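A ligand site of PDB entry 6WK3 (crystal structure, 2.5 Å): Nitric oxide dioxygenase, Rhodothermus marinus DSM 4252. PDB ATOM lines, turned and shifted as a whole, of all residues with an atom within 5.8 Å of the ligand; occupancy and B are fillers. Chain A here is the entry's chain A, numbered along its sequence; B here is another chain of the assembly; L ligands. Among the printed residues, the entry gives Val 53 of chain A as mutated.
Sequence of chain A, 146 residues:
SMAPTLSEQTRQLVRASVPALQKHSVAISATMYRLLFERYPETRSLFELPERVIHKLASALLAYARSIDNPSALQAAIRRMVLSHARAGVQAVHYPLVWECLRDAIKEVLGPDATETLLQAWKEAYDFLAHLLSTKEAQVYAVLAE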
ATOM      1  N   LEU A  36      29.290  32.392 -15.251  1.00  0.00           N
ATOM      2  CA  LEU A  36      28.397  33.063 -16.188  1.00  0.00           C
ATOM      3  C   LEU A  36      27.568  34.141 -15.479  1.00  0.00           C
ATOM      4  O   LEU A  36      27.340  35.224 -16.045  1.00  0.00           O
ATOM      5  CB  LEU A  36      27.482  32.036 -16.866  1.00  0.00           C
ATOM      6  CG  LEU A  36      26.524  32.499 -17.964  1.00  0.00           C
ATOM      7  CD1 LEU A  36      27.253  32.698 -19.272  1.00  0.00           C
ATOM      8  CD2 LEU A  36      25.382  31.504 -18.129  1.00  0.00           C
ATOM      9  N   THR A  43      22.676  37.557 -18.854  1.00  0.00           N
ATOM     10  CA  THR A  43      22.178  36.202 -19.030  1.00  0.00           C
ATOM     11  C   THR A  43      21.421  35.663 -17.823  1.00  0.00           C
ATOM     12  O   THR A  43      20.704  34.670 -17.971  1.00  0.00           O
ATOM     13  CB  THR A  43      23.334  35.238 -19.323  1.00  0.00           C
ATOM     14  OG1 THR A  43      24.124  35.053 -18.138  1.00  0.00           O
ATOM     15  CG2 THR A  43      24.211  35.758 -20.457  1.00  0.00           C
ATOM     16  N   LEU A  46      17.747  34.785 -17.938  1.00  0.00           N
ATOM     17  CA  LEU A  46      17.287  33.627 -18.689  1.00  0.00           C
ATOM     18  C   LEU A  46      16.944  32.432 -17.810  1.00  0.00           C
ATOM     19  O   LEU A  46      16.176  31.579 -18.243  1.00  0.00           O
ATOM     20  CB  LEU A  46      18.339  33.239 -19.729  1.00  0.00           C
ATOM     21  CG  LEU A  46      18.761  34.358 -20.687  1.00  0.00           C
ATOM     22  CD1 LEU A  46      19.938  33.924 -21.536  1.00  0.00           C
ATOM     23  CD2 LEU A  46      17.605  34.761 -21.571  1.00  0.00           C
ATOM     24  N   PHE A  47      17.484  32.362 -16.591  1.00  0.00           N
ATOM     25  CA  PHE A  47      17.386  31.166 -15.762  1.00  0.00           C
ATOM     26  C   PHE A  47      16.256  31.326 -14.736  1.00  0.00           C
ATOM     27  O   PHE A  47      16.417  32.024 -13.735  1.00  0.00           O
ATOM     28  CB  PHE A  47      18.715  30.880 -15.072  1.00  0.00           C
ATOM     29  CG  PHE A  47      19.808  30.536 -16.023  1.00  0.00           C
ATOM     30  CD1 PHE A  47      20.564  31.529 -16.628  1.00  0.00           C
ATOM     31  CD2 PHE A  47      20.097  29.219 -16.322  1.00  0.00           C
ATOM     32  CE1 PHE A  47      21.583  31.211 -17.507  1.00  0.00           C
ATOM     33  CE2 PHE A  47      21.113  28.895 -17.195  1.00  0.00           C
ATOM     34  CZ  PHE A  47      21.850  29.894 -17.787  1.00  0.00           C
ATOM     35  N   GLU A  48      15.134  30.662 -14.992  1.00  0.00           N
ATOM     36  CA  GLU A  48      14.048  30.618 -14.017  1.00  0.00           C
ATOM     37  C   GLU A  48      14.446  29.816 -12.780  1.00  0.00           C
ATOM     38  O   GLU A  48      14.275  30.267 -11.641  1.00  0.00           O
ATOM     39  CB  GLU A  48      12.787  30.014 -14.646  1.00  0.00           C
ATOM     40  CG  GLU A  48      11.924  30.990 -15.443  1.00  0.00           C
ATOM     41  CD  GLU A  48      10.527  30.441 -15.744  1.00  0.00           C
ATOM     42  OE1 GLU A  48      10.275  29.233 -15.525  1.00  0.00           O
ATOM     43  OE2 GLU A  48       9.675  31.226 -16.222  1.00  0.00           O
ATOM     44  N   VAL A  53      18.596  23.708 -13.342  1.00  0.00           N
ATOM     45  CA  VAL A  53      19.311  23.638 -14.613  1.00  0.00           C
ATOM     46  C   VAL A  53      20.735  23.162 -14.397  1.00  0.00           C
ATOM     47  O   VAL A  53      21.305  22.467 -15.253  1.00  0.00           O
ATOM     48  CB  VAL A  53      19.268  25.022 -15.299  1.00  0.00           C
ATOM     49  CG1 VAL A  53      20.150  25.054 -16.525  1.00  0.00           C
ATOM     50  CG2 VAL A  53      17.827  25.377 -15.663  1.00  0.00           C
ATOM     51  N   LYS A  56      20.743  19.449 -14.393  1.00  0.00           N
ATOM     52  CA  LYS A  56      20.417  18.958 -15.726  1.00  0.00           C
ATOM     53  C   LYS A  56      21.635  19.027 -16.652  1.00  0.00           C
ATOM     54  O   LYS A  56      21.916  18.077 -17.388  1.00  0.00           O
ATOM     55  CB  LYS A  56      19.260  19.758 -16.315  1.00  0.00           C
ATOM     56  CG  LYS A  56      17.892  19.253 -15.905  1.00  0.00           C
ATOM     57  CD  LYS A  56      16.804  20.231 -16.317  1.00  0.00           C
ATOM     58  CE  LYS A  56      15.535  19.500 -16.759  1.00  0.00           C
ATOM     59  NZ  LYS A  56      14.942  18.668 -15.690  1.00  0.00           N
ATOM     60  N   LEU A  57      22.356  20.154 -16.621  1.00  0.00           N
ATOM     61  CA  LEU A  57      23.552  20.280 -17.446  1.00  0.00           C
ATOM     62  C   LEU A  57      24.620  19.280 -17.020  1.00  0.00           C
ATOM     63  O   LEU A  57      25.308  18.707 -17.867  1.00  0.00           O
ATOM     64  CB  LEU A  57      24.092  21.707 -17.390  1.00  0.00           C
ATOM     65  CG  LEU A  57      25.361  21.884 -18.247  1.00  0.00           C
ATOM     66  CD1 LEU A  57      25.025  22.375 -19.647  1.00  0.00           C
ATOM     67  CD2 LEU A  57      26.357  22.827 -17.589  1.00  0.00           C
ATOM     68  N   ALA A  60      23.727  16.066 -18.591  1.00  0.00           N
ATOM     69  CA  ALA A  60      23.930  16.132 -20.037  1.00  0.00           C
ATOM     70  C   ALA A  60      25.405  16.010 -20.387  1.00  0.00           C
ATOM     71  O   ALA A  60      25.769  15.260 -21.301  1.00  0.00           O
ATOM     72  CB  ALA A  60      23.345  17.433 -20.588  1.00  0.00           C
ATOM     73  N   LEU A  61      26.277  16.732 -19.680  1.00  0.00           N
ATOM     74  CA  LEU A  61      27.704  16.588 -19.919  1.00  0.00           C
ATOM     75  C   LEU A  61      28.136  15.134 -19.769  1.00  0.00           C
ATOM     76  O   LEU A  61      28.828  14.590 -20.646  1.00  0.00           O
ATOM     77  CB  LEU A  61      28.498  17.485 -18.954  1.00  0.00           C
ATOM     78  CG  LEU A  61      28.399  18.989 -19.194  1.00  0.00           C
ATOM     79  CD1 LEU A  61      29.177  19.716 -18.110  1.00  0.00           C
ATOM     80  CD2 LEU A  61      28.893  19.380 -20.581  1.00  0.00           C
ATOM     81  N   ARG A  80      15.045  18.248 -26.098  1.00  0.00           N
ATOM     82  CA  ARG A  80      14.708  18.971 -24.879  1.00  0.00           C
ATOM     83  C   ARG A  80      15.541  20.236 -24.745  1.00  0.00           C
ATOM     84  O   ARG A  80      15.020  21.299 -24.407  1.00  0.00           O
ATOM     85  CB  ARG A  80      14.899  18.073 -23.653  1.00  0.00           C
ATOM     86  CG  ARG A  80      13.633  17.365 -23.213  1.00  0.00           C
ATOM     87  CD  ARG A  80      13.774  16.840 -21.791  1.00  0.00           C
ATOM     88  NE  ARG A  80      15.147  16.420 -21.507  1.00  0.00           N
ATOM     89  CZ  ARG A  80      15.643  15.207 -21.771  1.00  0.00           C
ATOM     90  NH1 ARG A  80      14.863  14.283 -22.325  1.00  0.00           N
ATOM     91  NH2 ARG A  80      16.903  14.919 -21.475  1.00  0.00           N
ATOM     92  N   MET A  81      16.853  20.138 -25.007  1.00  0.00           N
ATOM     93  CA  MET A  81      17.708  21.318 -24.910  1.00  0.00           C
ATOM     94  C   MET A  81      17.263  22.410 -25.870  1.00  0.00           C
ATOM     95  O   MET A  81      17.240  23.591 -25.506  1.00  0.00           O
ATOM     96  CB  MET A  81      19.164  20.942 -25.192  1.00  0.00           C
ATOM     97  CG  MET A  81      19.779  20.053 -24.135  1.00  0.00           C
ATOM     98  SD  MET A  81      21.420  19.503 -24.600  1.00  0.00           S
ATOM     99  CE  MET A  81      21.370  17.819 -24.001  1.00  0.00           C
ATOM    100  N   LEU A  83      14.269  23.052 -27.201  1.00  0.00           N
ATOM    101  CA  LEU A  83      13.009  23.688 -26.872  1.00  0.00           C
ATOM    102  C   LEU A  83      13.092  24.449 -25.566  1.00  0.00           C
ATOM    103  O   LEU A  83      12.466  25.510 -25.431  1.00  0.00           O
ATOM    104  CB  LEU A  83      11.895  22.644 -26.836  1.00  0.00           C
ATOM    105  CG  LEU A  83      11.753  21.895 -28.159  1.00  0.00           C
ATOM    106  CD1 LEU A  83      10.905  20.652 -28.018  1.00  0.00           C
ATOM    107  CD2 LEU A  83      11.180  22.821 -29.232  1.00  0.00           C
ATOM    108  N   SER A  84      13.873  23.953 -24.599  1.00  0.00           N
ATOM    109  CA  SER A  84      14.153  24.725 -23.402  1.00  0.00           C
ATOM    110  C   SER A  84      14.845  26.035 -23.740  1.00  0.00           C
ATOM    111  O   SER A  84      14.442  27.109 -23.264  1.00  0.00           O
ATOM    112  CB  SER A  84      14.995  23.898 -22.429  1.00  0.00           C
ATOM    113  OG  SER A  84      14.302  22.723 -22.033  1.00  0.00           O
ATOM    114  N   HIS A  85      15.887  25.987 -24.571  1.00  0.00           N
ATOM    115  CA  HIS A  85      16.603  27.199 -24.946  1.00  0.00           C
ATOM    116  C   HIS A  85      15.684  28.187 -25.644  1.00  0.00           C
ATOM    117  O   HIS A  85      15.679  29.383 -25.335  1.00  0.00           O
ATOM    118  CB  HIS A  85      17.774  26.871 -25.854  1.00  0.00           C
ATOM    119  CG  HIS A  85      18.922  26.234 -25.130  1.00  0.00           C
ATOM    120  ND1 HIS A  85      19.987  25.663 -25.792  1.00  0.00           N
ATOM    121  CD2 HIS A  85      19.158  26.079 -23.814  1.00  0.00           C
ATOM    122  CE1 HIS A  85      20.841  25.183 -24.898  1.00  0.00           C
ATOM    123  NE2 HIS A  85      20.357  25.421 -23.701  1.00  0.00           N
ATOM    124  N   ARG A  87      12.493  28.389 -25.441  1.00  0.00           N
ATOM    125  CA  ARG A  87      11.544  28.900 -24.449  1.00  0.00           C
ATOM    126  C   ARG A  87      12.129  30.075 -23.677  1.00  0.00           C
ATOM    127  O   ARG A  87      11.423  31.049 -23.393  1.00  0.00           O
ATOM    128  CB  ARG A  87      11.143  27.774 -23.487  1.00  0.00           C
ATOM    129  CG  ARG A  87      10.160  28.206 -22.409  1.00  0.00           C
ATOM    130  CD  ARG A  87       9.608  27.006 -21.645  1.00  0.00           C
ATOM    131  NE  ARG A  87      10.661  26.254 -20.975  1.00  0.00           N
ATOM    132  CZ  ARG A  87      10.468  25.091 -20.368  1.00  0.00           C
ATOM    133  NH1 ARG A  87       9.271  24.533 -20.348  1.00  0.00           N
ATOM    134  NH2 ARG A  87      11.490  24.472 -19.770  1.00  0.00           N
ATOM    135  N   ALA A  88      13.421  30.013 -23.344  1.00  0.00           N
ATOM    136  CA  ALA A  88      14.046  31.062 -22.535  1.00  0.00           C
ATOM    137  C   ALA A  88      14.685  32.179 -23.349  1.00  0.00           C
ATOM    138  O   ALA A  88      15.130  33.166 -22.769  1.00  0.00           O
ATOM    139  CB  ALA A  88      15.104  30.445 -21.610  1.00  0.00           C
ATOM    140  N   VAL A  90      17.409  31.835 -25.492  1.00  0.00           N
ATOM    141  CA  VAL A  90      18.841  31.691 -25.680  1.00  0.00           C
ATOM    142  C   VAL A  90      19.195  32.015 -27.121  1.00  0.00           C
ATOM    143  O   VAL A  90      18.491  31.643 -28.063  1.00  0.00           O
ATOM    144  CB  VAL A  90      19.303  30.274 -25.295  1.00  0.00           C
ATOM    145  CG1 VAL A  90      20.741  30.038 -25.716  1.00  0.00           C
ATOM    146  CG2 VAL A  90      19.130  30.075 -23.794  1.00  0.00           C
ATOM    147  N   GLN A  91      20.305  32.741 -27.300  1.00  0.00           N
ATOM    148  CA  GLN A  91      20.679  33.306 -28.581  1.00  0.00           C
ATOM    149  C   GLN A  91      21.996  32.713 -29.056  1.00  0.00           C
ATOM    150  O   GLN A  91      22.785  32.196 -28.271  1.00  0.00           O
ATOM    151  CB  GLN A  91      20.792  34.837 -28.502  1.00  0.00           C
ATOM    152  CG  GLN A  91      19.465  35.549 -28.282  1.00  0.00           C
ATOM    153  CD  GLN A  91      18.433  35.212 -29.356  1.00  0.00           C
ATOM    154  OE1 GLN A  91      18.773  34.984 -30.520  1.00  0.00           O
ATOM    155  NE2 GLN A  91      17.163  35.169 -28.959  1.00  0.00           N
ATOM    156  N   HIS A  94      25.221  33.746 -27.369  1.00  0.00           N
ATOM    157  CA  HIS A  94      25.490  33.317 -25.997  1.00  0.00           C
ATOM    158  C   HIS A  94      26.452  32.137 -25.948  1.00  0.00           C
ATOM    159  O   HIS A  94      27.178  31.979 -24.959  1.00  0.00           O
ATOM    160  CB  HIS A  94      24.176  32.941 -25.297  1.00  0.00           C
ATOM    161  CG  HIS A  94      23.281  34.116 -25.011  1.00  0.00           C
ATOM    162  ND1 HIS A  94      21.929  34.098 -25.273  1.00  0.00           N
ATOM    163  CD2 HIS A  94      23.554  35.333 -24.484  1.00  0.00           C
ATOM    164  CE1 HIS A  94      21.399  35.260 -24.923  1.00  0.00           C
ATOM    165  NE2 HIS A  94      22.363  36.019 -24.447  1.00  0.00           N
ATOM    166  N   TYR A  95      26.466  31.308 -26.992  1.00  0.00           N
ATOM    167  CA  TYR A  95      27.250  30.074 -26.952  1.00  0.00           C
ATOM    168  C   TYR A  95      28.733  30.293 -26.728  1.00  0.00           C
ATOM    169  O   TYR A  95      29.341  29.509 -25.973  1.00  0.00           O
ATOM    170  CB  TYR A  95      26.985  29.252 -28.214  1.00  0.00           C
ATOM    171  CG  TYR A  95      25.647  28.563 -28.161  1.00  0.00           C
ATOM    172  CD1 TYR A  95      25.511  27.323 -27.530  1.00  0.00           C
ATOM    173  CD2 TYR A  95      24.503  29.151 -28.681  1.00  0.00           C
ATOM    174  CE1 TYR A  95      24.294  26.701 -27.450  1.00  0.00           C
ATOM    175  CE2 TYR A  95      23.276  28.529 -28.605  1.00  0.00           C
ATOM    176  CZ  TYR A  95      23.184  27.297 -27.991  1.00  0.00           C
ATOM    177  OH  TYR A  95      21.963  26.667 -27.905  1.00  0.00           O
ATOM    178  N   VAL A  98      29.180  30.777 -22.842  1.00  0.00           N
ATOM    179  CA  VAL A  98      29.071  29.602 -21.994  1.00  0.00           C
ATOM    180  C   VAL A  98      30.271  28.682 -22.181  1.00  0.00           C
ATOM    181  O   VAL A  98      30.707  28.007 -21.245  1.00  0.00           O
ATOM    182  CB  VAL A  98      27.739  28.870 -22.260  1.00  0.00           C
ATOM    183  CG1 VAL A  98      27.734  27.485 -21.632  1.00  0.00           C
ATOM    184  CG2 VAL A  98      26.594  29.700 -21.712  1.00  0.00           C
ATOM    185  N   TYR A 126      32.246  20.711 -27.495  1.00  0.00           N
ATOM    186  CA  TYR A 126      31.297  21.779 -27.232  1.00  0.00           C
ATOM    187  C   TYR A 126      30.842  22.431 -28.526  1.00  0.00           C
ATOM    188  O   TYR A 126      29.644  22.679 -28.725  1.00  0.00           O
ATOM    189  CB  TYR A 126      31.908  22.821 -26.294  1.00  0.00           C
ATOM    190  CG  TYR A 126      30.981  23.967 -26.010  1.00  0.00           C
ATOM    191  CD1 TYR A 126      30.944  25.082 -26.841  1.00  0.00           C
ATOM    192  CD2 TYR A 126      30.108  23.934 -24.925  1.00  0.00           C
ATOM    193  CE1 TYR A 126      30.083  26.123 -26.610  1.00  0.00           C
ATOM    194  CE2 TYR A 126      29.249  24.975 -24.677  1.00  0.00           C
ATOM    195  CZ  TYR A 126      29.241  26.070 -25.517  1.00  0.00           C
ATOM    196  OH  TYR A 126      28.375  27.111 -25.257  1.00  0.00           O
ATOM    197  N   LEU A 129      28.264  20.331 -30.344  1.00  0.00           N
ATOM    198  CA  LEU A 129      26.944  20.386 -29.715  1.00  0.00           C
ATOM    199  C   LEU A 129      26.338  21.779 -29.817  1.00  0.00           C
ATOM    200  O   LEU A 129      25.131  21.913 -30.037  1.00  0.00           O
ATOM    201  CB  LEU A 129      27.060  19.953 -28.251  1.00  0.00           C
ATOM    202  CG  LEU A 129      25.769  19.613 -27.513  1.00  0.00           C
ATOM    203  CD1 LEU A 129      24.854  18.741 -28.383  1.00  0.00           C
ATOM    204  CD2 LEU A 129      26.110  18.916 -26.218  1.00  0.00           C
ATOM    205  N   ALA A 130      27.161  22.824 -29.698  1.00  0.00           N
ATOM    206  CA  ALA A 130      26.668  24.192 -29.818  1.00  0.00           C
ATOM    207  C   ALA A 130      26.116  24.466 -31.210  1.00  0.00           C
ATOM    208  O   ALA A 130      25.051  25.078 -31.355  1.00  0.00           O
ATOM    209  CB  ALA A 130      27.780  25.187 -29.475  1.00  0.00           C
ATOM    210  N   LEU A 133      22.774  22.705 -31.556  1.00  0.00           N
ATOM    211  CA  LEU A 133      21.714  23.318 -30.761  1.00  0.00           C
ATOM    212  C   LEU A 133      21.311  24.673 -31.332  1.00  0.00           C
ATOM    213  O   LEU A 133      20.124  24.984 -31.451  1.00  0.00           O
ATOM    214  CB  LEU A 133      22.168  23.458 -29.314  1.00  0.00           C
ATOM    215  CG  LEU A 133      22.304  22.154 -28.550  1.00  0.00           C
ATOM    216  CD1 LEU A 133      22.664  22.420 -27.104  1.00  0.00           C
ATOM    217  CD2 LEU A 133      21.024  21.339 -28.660  1.00  0.00           C
ATOM    218  N   GLU B  48       6.746  17.537 -15.180  1.00  0.00           N
ATOM    219  CA  GLU B  48       7.905  17.495 -14.298  1.00  0.00           C
ATOM    220  C   GLU B  48       7.635  18.248 -12.993  1.00  0.00           C
ATOM    221  O   GLU B  48       7.960  17.756 -11.906  1.00  0.00           O
ATOM    222  CB  GLU B  48       9.127  18.102 -15.006  1.00  0.00           C
ATOM    223  CG  GLU B  48       9.993  17.096 -15.742  1.00  0.00           C
ATOM    224  CD  GLU B  48      11.006  17.761 -16.654  1.00  0.00           C
ATOM    225  OE1 GLU B  48      11.279  17.207 -17.745  1.00  0.00           O
ATOM    226  OE2 GLU B  48      11.510  18.842 -16.291  1.00  0.00           O
ATOM    227  N   ARG B  87       8.279  20.581 -25.721  1.00  0.00           N
ATOM    228  CA  ARG B  87       9.324  20.027 -24.859  1.00  0.00           C
ATOM    229  C   ARG B  87       8.818  18.857 -24.037  1.00  0.00           C
ATOM    230  O   ARG B  87       9.602  17.970 -23.679  1.00  0.00           O
ATOM    231  CB  ARG B  87       9.872  21.124 -23.955  1.00  0.00           C
ATOM    232  CG  ARG B  87      11.006  20.692 -23.051  1.00  0.00           C
ATOM    233  CD  ARG B  87      11.117  21.609 -21.824  1.00  0.00           C
ATOM    234  NE  ARG B  87      12.014  21.024 -20.835  1.00  0.00           N
ATOM    235  CZ  ARG B  87      11.663  20.069 -19.973  1.00  0.00           C
ATOM    236  NH1 ARG B  87      10.426  19.602 -19.967  1.00  0.00           N
ATOM    237  NH2 ARG B  87      12.559  19.597 -19.112  1.00  0.00           N
HETATM  238  C1  LIG L   1      18.691  24.561 -20.212  1.00  0.00           C
HETATM  239  C2  LIG L   1      22.560  22.144 -21.898  1.00  0.00           C
HETATM  240  C3  LIG L   1      24.026  26.284 -23.927  1.00  0.00           C
HETATM  241  C4  LIG L   1      21.073  28.725 -20.942  1.00  0.00           C
HETATM  242  C5  LIG L   1      19.561  23.541 -20.542  1.00  0.00           C
HETATM  243  C6  LIG L   1      19.365  22.129 -20.270  1.00  0.00           C
HETATM  244  C7  LIG L   1      20.434  21.467 -20.729  1.00  0.00           C
HETATM  245  C8  LIG L   1      21.350  22.421 -21.312  1.00  0.00           C
HETATM  246  C9  LIG L   1      20.655  19.938 -20.648  1.00  0.00           C
HETATM  247  C10 LIG L   1      18.141  21.508 -19.579  1.00  0.00           C
HETATM  248  C11 LIG L   1      17.118  21.157 -20.649  1.00  0.00           C
HETATM  249  C12 LIG L   1      15.988  20.368 -20.038  1.00  0.00           C
HETATM  250  O1  LIG L   1      14.954  20.981 -19.681  1.00  0.00           O
HETATM  251  O2  LIG L   1      16.126  19.134 -19.902  1.00  0.00           O
HETATM  252  C13 LIG L   1      23.286  23.037 -22.651  1.00  0.00           C
HETATM  253  C14 LIG L   1      24.437  22.744 -23.481  1.00  0.00           C
HETATM  254  C15 LIG L   1      24.850  23.898 -24.031  1.00  0.00           C
HETATM  255  C16 LIG L   1      23.960  24.946 -23.583  1.00  0.00           C
HETATM  256  C17 LIG L   1      25.036  21.329 -23.634  1.00  0.00           C
HETATM  257  C18 LIG L   1      26.020  24.157 -25.023  1.00  0.00           C
HETATM  258  C19 LIG L   1      26.557  23.206 -25.787  1.00  0.00           C
HETATM  259  C20 LIG L   1      23.392  27.317 -23.280  1.00  0.00           C
HETATM  260  C21 LIG L   1      23.592  28.729 -23.518  1.00  0.00           C
HETATM  261  C22 LIG L   1      22.801  29.412 -22.695  1.00  0.00           C
HETATM  262  C23 LIG L   1      22.035  28.469 -21.908  1.00  0.00           C
HETATM  263  C24 LIG L   1      24.578  29.323 -24.542  1.00  0.00           C
HETATM  264  C25 LIG L   1      22.741  30.960 -22.654  1.00  0.00           C
HETATM  265  C26 LIG L   1      22.407  31.605 -21.539  1.00  0.00           C
HETATM  266  C27 LIG L   1      20.075  27.839 -20.566  1.00  0.00           C
HETATM  267  C28 LIG L   1      18.791  28.143 -19.971  1.00  0.00           C
HETATM  268  C29 LIG L   1      18.137  26.975 -19.771  1.00  0.00           C
HETATM  269  C30 LIG L   1      18.990  25.905 -20.233  1.00  0.00           C
HETATM  270  C31 LIG L   1      18.279  29.560 -19.624  1.00  0.00           C
HETATM  271  C32 LIG L   1      16.740  26.746 -19.156  1.00  0.00           C
HETATM  272  C33 LIG L   1      15.655  27.150 -20.147  1.00  0.00           C
HETATM  273  C34 LIG L   1      14.338  26.512 -19.782  1.00  0.00           C
HETATM  274  O3  LIG L   1      14.333  25.431 -19.126  1.00  0.00           O
HETATM  275  O4  LIG L   1      13.283  27.073 -20.173  1.00  0.00           O
HETATM  276  N1  LIG L   1      20.782  23.674 -21.167  1.00  0.00           N
HETATM  277  N2  LIG L   1      23.027  24.382 -22.738  1.00  0.00           N
HETATM  278  N3  LIG L   1      22.425  27.205 -22.289  1.00  0.00           N
HETATM  279  N4  LIG L   1      20.152  26.476 -20.708  1.00  0.00           N
HETATM  280 FE1  LIG L   1      21.659  25.448 -21.632  1.00  0.00          FE
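OG of Ser 84 is in hydrogen-bond range of O1 of the ligand, at 3.0 Å. NH2 of Arg 87 of chain B lies within salt-bridge range of O1 of the ligand (2.8 Å). NE of Arg 80 is in salt-bridge range of O2 of the ligand (3.3 Å). NE2 of His 85 is bound to FE1 of the ligand, at 2.4 Å. O4 of the ligand is in salt-bridge range of NE of Arg 87 of chain A, 2.9 Å away.
Merely in contact with the ligand: Lys 56 (3.2 Å), Leu 46 (3.2 Å), Leu 57 (3.3 Å), Tyr 126 (3.3 Å), Phe 47 (3.5 Å), Val 98 (3.5 Å), Tyr 95 (3.6 Å), Met 81 (3.6 Å), His 94 (3.6 Å), Ala 88 (3.6 Å), Ala 60 (3.7 Å), Leu 129 (3.7 Å), Val 90 (3.7 Å), Val 53 (3.9 Å) and Ala 130 (3.98 Å).
NH2 of Arg 87 of chain B lies within salt-bridge range of OE1 of Glu 48 of chain B (3.0 Å). ND1 of His 85 lies close to O of Met 81 (3.5 Å). A ring nitrogen (ND1) of His 94 lies within hydrogen-bond range of the backbone NH (N) of Gln 91. OG of Ser 84 is in hydrogen-bond range of O of Arg 80, at 2.9 Å. NE of Arg 87 of chain B is in hydrogen-bond range of OG of Ser 84, at 3.1 Å. The side-chain amino group of Lys 56 is in salt-bridge range of the side-chain carboxylate of Glu 48 of chain B (3.5 Å). O of His 85 is in hydrogen-bond range of N of Val 90, at 3.0 Å. The backbone carbonyl oxygen of Tyr 95 sits at hydrogen-bond distance from the side-chain hydroxyl of Tyr 126 (2.7 Å).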
